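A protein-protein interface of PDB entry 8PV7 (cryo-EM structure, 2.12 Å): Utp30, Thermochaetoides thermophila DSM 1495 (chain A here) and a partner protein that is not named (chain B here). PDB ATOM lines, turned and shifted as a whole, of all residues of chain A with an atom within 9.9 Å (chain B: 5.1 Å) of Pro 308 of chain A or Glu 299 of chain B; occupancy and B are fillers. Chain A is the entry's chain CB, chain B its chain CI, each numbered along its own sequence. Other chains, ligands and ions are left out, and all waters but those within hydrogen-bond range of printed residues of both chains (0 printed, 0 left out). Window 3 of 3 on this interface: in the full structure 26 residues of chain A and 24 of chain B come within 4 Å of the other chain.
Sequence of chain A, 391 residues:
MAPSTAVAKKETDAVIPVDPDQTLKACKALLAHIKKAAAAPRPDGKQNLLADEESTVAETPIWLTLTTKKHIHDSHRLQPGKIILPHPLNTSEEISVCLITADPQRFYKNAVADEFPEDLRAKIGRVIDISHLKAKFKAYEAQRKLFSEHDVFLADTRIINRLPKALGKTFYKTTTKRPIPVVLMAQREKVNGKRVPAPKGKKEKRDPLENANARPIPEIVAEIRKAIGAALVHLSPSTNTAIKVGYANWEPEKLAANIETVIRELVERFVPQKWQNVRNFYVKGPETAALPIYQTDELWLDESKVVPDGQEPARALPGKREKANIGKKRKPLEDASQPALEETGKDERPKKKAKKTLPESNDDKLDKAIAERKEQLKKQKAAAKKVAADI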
ATOM      1  N   TRP A 300       4.374  17.361  -3.377  1.00  0.00           N
ATOM      2  CA  TRP A 300       5.720  17.795  -3.044  1.00  0.00           C
ATOM      3  C   TRP A 300       6.697  17.365  -4.126  1.00  0.00           C
ATOM      4  O   TRP A 300       6.432  16.441  -4.899  1.00  0.00           O
ATOM      5  CB  TRP A 300       6.174  17.240  -1.693  1.00  0.00           C
ATOM      6  CG  TRP A 300       5.909  15.789  -1.500  1.00  0.00           C
ATOM      7  CD1 TRP A 300       6.729  14.754  -1.832  1.00  0.00           C
ATOM      8  CD2 TRP A 300       4.752  15.208  -0.895  1.00  0.00           C
ATOM      9  NE1 TRP A 300       6.148  13.561  -1.487  1.00  0.00           N
ATOM     10  CE2 TRP A 300       4.932  13.813  -0.908  1.00  0.00           C
ATOM     11  CE3 TRP A 300       3.576  15.730  -0.349  1.00  0.00           C
ATOM     12  CZ2 TRP A 300       3.985  12.935  -0.392  1.00  0.00           C
ATOM     13  CZ3 TRP A 300       2.636  14.858   0.158  1.00  0.00           C
ATOM     14  CH2 TRP A 300       2.844  13.476   0.131  1.00  0.00           C
ATOM     15  N   ASP A 302       9.920  16.174  -3.619  1.00  0.00           N
ATOM     16  CA  ASP A 302      10.584  14.935  -3.240  1.00  0.00           C
ATOM     17  C   ASP A 302      10.431  14.756  -1.737  1.00  0.00           C
ATOM     18  O   ASP A 302       9.698  15.494  -1.074  1.00  0.00           O
ATOM     19  CB  ASP A 302      12.055  14.940  -3.663  1.00  0.00           C
ATOM     20  CG  ASP A 302      12.825  16.104  -3.080  1.00  0.00           C
ATOM     21  OD1 ASP A 302      12.193  17.122  -2.729  1.00  0.00           O
ATOM     22  OD2 ASP A 302      14.065  16.004  -2.972  1.00  0.00           O
ATOM     23  N   GLU A 303      11.137  13.761  -1.202  1.00  0.00           N
ATOM     24  CA  GLU A 303      11.088  13.494   0.228  1.00  0.00           C
ATOM     25  C   GLU A 303      11.876  14.509   1.041  1.00  0.00           C
ATOM     26  O   GLU A 303      11.679  14.594   2.258  1.00  0.00           O
ATOM     27  CB  GLU A 303      11.608  12.085   0.515  1.00  0.00           C
ATOM     28  CG  GLU A 303      10.851  10.998  -0.226  1.00  0.00           C
ATOM     29  CD  GLU A 303       9.397  10.913   0.190  1.00  0.00           C
ATOM     30  OE1 GLU A 303       8.539  10.686  -0.688  1.00  0.00           O
ATOM     31  OE2 GLU A 303       9.110  11.069   1.396  1.00  0.00           O
ATOM     32  N   SER A 304      12.762  15.277   0.401  1.00  0.00           N
ATOM     33  CA  SER A 304      13.471  16.335   1.111  1.00  0.00           C
ATOM     34  C   SER A 304      12.541  17.482   1.475  1.00  0.00           C
ATOM     35  O   SER A 304      12.802  18.211   2.437  1.00  0.00           O
ATOM     36  CB  SER A 304      14.639  16.842   0.268  1.00  0.00           C
ATOM     37  OG  SER A 304      14.246  17.943  -0.531  1.00  0.00           O
ATOM     38  N   LYS A 305      11.459  17.664   0.714  1.00  0.00           N
ATOM     39  CA  LYS A 305      10.471  18.679   1.064  1.00  0.00           C
ATOM     40  C   LYS A 305       9.695  18.281   2.313  1.00  0.00           C
ATOM     41  O   LYS A 305       9.223  19.144   3.061  1.00  0.00           O
ATOM     42  CB  LYS A 305       9.520  18.916  -0.108  1.00  0.00           C
ATOM     43  CG  LYS A 305      10.195  19.413  -1.379  1.00  0.00           C
ATOM     44  CD  LYS A 305      11.162  20.551  -1.096  1.00  0.00           C
ATOM     45  CE  LYS A 305      12.376  20.483  -2.003  1.00  0.00           C
ATOM     46  NZ  LYS A 305      13.251  21.677  -1.841  1.00  0.00           N
ATOM     47  N   VAL A 306       9.533  16.981   2.544  1.00  0.00           N
ATOM     48  CA  VAL A 306       8.864  16.504   3.749  1.00  0.00           C
ATOM     49  C   VAL A 306       9.897  16.446   4.870  1.00  0.00           C
ATOM     50  O   VAL A 306      10.774  15.578   4.873  1.00  0.00           O
ATOM     51  CB  VAL A 306       8.206  15.139   3.526  1.00  0.00           C
ATOM     52  CG1 VAL A 306       7.119  14.904   4.557  1.00  0.00           C
ATOM     53  CG2 VAL A 306       7.640  15.050   2.118  1.00  0.00           C
ATOM     54  N   VAL A 307       9.801  17.370   5.821  1.00  0.00           N
ATOM     55  CA  VAL A 307      10.728  17.410   6.947  1.00  0.00           C
ATOM     56  C   VAL A 307       9.898  17.367   8.227  1.00  0.00           C
ATOM     57  O   VAL A 307       8.771  17.887   8.252  1.00  0.00           O
ATOM     58  CB  VAL A 307      11.657  18.642   6.854  1.00  0.00           C
ATOM     59  CG1 VAL A 307      11.039  19.898   7.466  1.00  0.00           C
ATOM     60  CG2 VAL A 307      13.023  18.354   7.465  1.00  0.00           C
ATOM     61  N   PRO A 308      10.366  16.697   9.291  1.00  0.00           N
ATOM     62  CA  PRO A 308       9.592  16.700  10.534  1.00  0.00           C
ATOM     63  C   PRO A 308      10.122  17.698  11.556  1.00  0.00           C
ATOM     64  O   PRO A 308       9.424  17.968  12.532  1.00  0.00           O
ATOM     65  CB  PRO A 308       9.746  15.266  11.046  1.00  0.00           C
ATOM     66  CG  PRO A 308      11.010  14.751  10.415  1.00  0.00           C
ATOM     67  CD  PRO A 308      11.433  15.683   9.313  1.00  0.00           C
ATOM     68  N   LEU B 297       8.407  22.097   3.940  1.00  0.00           N
ATOM     69  CA  LEU B 297       7.382  22.313   4.951  1.00  0.00           C
ATOM     70  C   LEU B 297       7.188  21.045   5.774  1.00  0.00           C
ATOM     71  O   LEU B 297       7.695  19.974   5.435  1.00  0.00           O
ATOM     72  CB  LEU B 297       6.031  22.739   4.340  1.00  0.00           C
ATOM     73  CG  LEU B 297       5.718  24.148   3.809  1.00  0.00           C
ATOM     74  CD1 LEU B 297       6.753  24.739   2.878  1.00  0.00           C
ATOM     75  CD2 LEU B 297       4.359  24.160   3.144  1.00  0.00           C
ATOM     76  N   SER B 298       6.440  21.184   6.868  1.00  0.00           N
ATOM     77  CA  SER B 298       6.217  20.080   7.790  1.00  0.00           C
ATOM     78  C   SER B 298       4.985  19.270   7.403  1.00  0.00           C
ATOM     79  O   SER B 298       4.264  19.603   6.456  1.00  0.00           O
ATOM     80  CB  SER B 298       6.062  20.599   9.219  1.00  0.00           C
ATOM     81  OG  SER B 298       7.220  21.301   9.631  1.00  0.00           O
ATOM     82  N   GLU B 299       4.746  18.196   8.166  1.00  0.00           N
ATOM     83  CA  GLU B 299       3.629  17.295   7.885  1.00  0.00           C
ATOM     84  C   GLU B 299       2.286  17.987   8.062  1.00  0.00           C
ATOM     85  O   GLU B 299       1.355  17.742   7.290  1.00  0.00           O
ATOM     86  CB  GLU B 299       3.708  16.055   8.779  1.00  0.00           C
ATOM     87  CG  GLU B 299       4.520  14.840   8.260  1.00  0.00           C
ATOM     88  CD  GLU B 299       6.023  15.058   8.021  1.00  0.00           C
ATOM     89  OE1 GLU B 299       6.531  16.197   8.034  1.00  0.00           O
ATOM     90  OE2 GLU B 299       6.717  14.039   7.812  1.00  0.00           O
ATOM     91  N   SER B 300       2.159  18.844   9.076  1.00  0.00           N
ATOM     92  CA  SER B 300       0.904  19.563   9.285  1.00  0.00           C
ATOM     93  C   SER B 300       0.636  20.546   8.150  1.00  0.00           C
ATOM     94  O   SER B 300      -0.511  20.717   7.712  1.00  0.00           O
ATOM     95  CB  SER B 300       0.936  20.286  10.630  1.00  0.00           C
ATOM     96  OG  SER B 300      -0.257  21.019  10.843  1.00  0.00           O
ATOM     97  N   GLN B 301       1.688  21.212   7.669  1.00  0.00           N
ATOM     98  CA  GLN B 301       1.540  22.122   6.539  1.00  0.00           C
ATOM     99  C   GLN B 301       1.172  21.377   5.261  1.00  0.00           C
ATOM    100  O   GLN B 301       0.312  21.837   4.495  1.00  0.00           O
ATOM    101  CB  GLN B 301       2.821  22.937   6.369  1.00  0.00           C
ATOM    102  CG  GLN B 301       2.959  24.027   7.423  1.00  0.00           C
ATOM    103  CD  GLN B 301       4.378  24.210   7.922  1.00  0.00           C
ATOM    104  OE1 GLN B 301       5.335  24.136   7.157  1.00  0.00           O
ATOM    105  NE2 GLN B 301       4.518  24.456   9.219  1.00  0.00           N
ATOM    106  N   TRP B 302       1.778  20.210   5.030  1.00  0.00           N
ATOM    107  CA  TRP B 302       1.374  19.392   3.892  1.00  0.00           C
ATOM    108  C   TRP B 302      -0.050  18.876   4.069  1.00  0.00           C
ATOM    109  O   TRP B 302      -0.783  18.703   3.092  1.00  0.00           O
ATOM    110  CB  TRP B 302       2.354  18.233   3.697  1.00  0.00           C
ATOM    111  CG  TRP B 302       3.670  18.642   3.090  1.00  0.00           C
ATOM    112  CD1 TRP B 302       4.903  18.518   3.658  1.00  0.00           C
ATOM    113  CD2 TRP B 302       3.883  19.244   1.804  1.00  0.00           C
ATOM    114  NE1 TRP B 302       5.868  19.002   2.812  1.00  0.00           N
ATOM    115  CE2 TRP B 302       5.269  19.452   1.667  1.00  0.00           C
ATOM    116  CE3 TRP B 302       3.039  19.623   0.757  1.00  0.00           C
ATOM    117  CZ2 TRP B 302       5.827  20.025   0.530  1.00  0.00           C
ATOM    118  CZ3 TRP B 302       3.597  20.190  -0.373  1.00  0.00           C
ATOM    119  CH2 TRP B 302       4.977  20.387  -0.476  1.00  0.00           C
ATOM    120  N   GLN B 303      -0.471  18.669   5.320  1.00  0.00           N
ATOM    121  CA  GLN B 303      -1.834  18.228   5.605  1.00  0.00           C
ATOM    122  C   GLN B 303      -2.859  19.292   5.238  1.00  0.00           C
ATOM    123  O   GLN B 303      -3.874  18.990   4.595  1.00  0.00           O
ATOM    124  CB  GLN B 303      -1.957  17.868   7.087  1.00  0.00           C
ATOM    125  CG  GLN B 303      -2.692  16.574   7.405  1.00  0.00           C
ATOM    126  CD  GLN B 303      -2.273  15.403   6.540  1.00  0.00           C
ATOM    127  OE1 GLN B 303      -1.084  15.165   6.312  1.00  0.00           O
ATOM    128  NE2 GLN B 303      -3.254  14.653   6.062  1.00  0.00           N
ATOM    129  N   PRO B 335       1.283  12.546   3.615  1.00  0.00           N
ATOM    130  CA  PRO B 335       2.611  12.209   4.132  1.00  0.00           C
ATOM    131  C   PRO B 335       2.577  11.778   5.595  1.00  0.00           C
ATOM    132  O   PRO B 335       2.642  10.581   5.873  1.00  0.00           O
ATOM    133  CB  PRO B 335       3.379  13.518   3.970  1.00  0.00           C
ATOM    134  CG  PRO B 335       2.334  14.554   4.175  1.00  0.00           C
ATOM    135  CD  PRO B 335       1.095  14.005   3.515  1.00  0.00           C
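The backbone NH (N) of Leu 297 of chain B sits at hydrogen-bond distance from the backbone carbonyl oxygen (O) of Lys 305 of chain A (3.2 Å).
O of Lys 305 of chain A sits at hydrogen-bond distance from NE1 of Trp 302 of chain B, at 3.4 Å.
N of Val 307 of chain A sits at hydrogen-bond distance from O of Leu 297 of chain B (3.4 Å).
The side-chain carboxylate of Glu 299 of chain B sits close to the backbone carbonyl oxygen of Val 307 of chain A, at 2.8 Å.
O of Leu 297 of chain B is in hydrogen-bond range of NE1 of Trp 302 of chain B (3.3 Å).
The side-chain amide oxygen (OE1) of Gln 301 of chain B sits at hydrogen-bond distance from the backbone NH (N) of Ser 298 of chain B.
Trp 300 of chain A touches Trp 302 of chain B (CB to CH2, 3.6 Å).
Trp 300 of chain A touches Pro 335 of chain B.
Val 306 of chain A touches Glu 299 of chain B.
CA of Ser 298 of chain B touches O of Val 307 of chain A (3.4 Å).
Glu 299 of chain B touches Pro 308 of chain A (OE1 to CA, 3.98 Å).
Of the printed residues of chain B, Pro 308 of chain A touches Glu 299.
Printed residues of chain A within 4 Å of Glu 299 of chain B: Val 306 (3.4 Å), Val 307 (2.8 Å) and Pro 308 (3.98 Å).
Ser 298 of chain B touches one residue of chain A.
No residue of chain A comes within 4 Å of Ser 300 of chain B.
Of the printed residues of chain A, Pro 335 of chain B touches Trp 300.
Of the printed residues of chain A, Trp 302 of chain B touches Trp 300 (3.6 Å) and Lys 305 (3.4 Å).
Gln 301 of chain B touches none of the printed residues of chain A.
The nearest printed residue of chain A that does not touch Glu 299 of chain B is Lys 305 of chain A (6.4 Å).
The nearest printed residue of chain B that does not touch Val 306 of chain A is Trp 302 of chain B (4.01 Å).
Of the 8 printed residues of chain B, 5 touch a printed residue of chain A.
Hydrophobic or aromatic side chains of chain B that line the printed part of chain A: Trp 302 and Pro 335.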
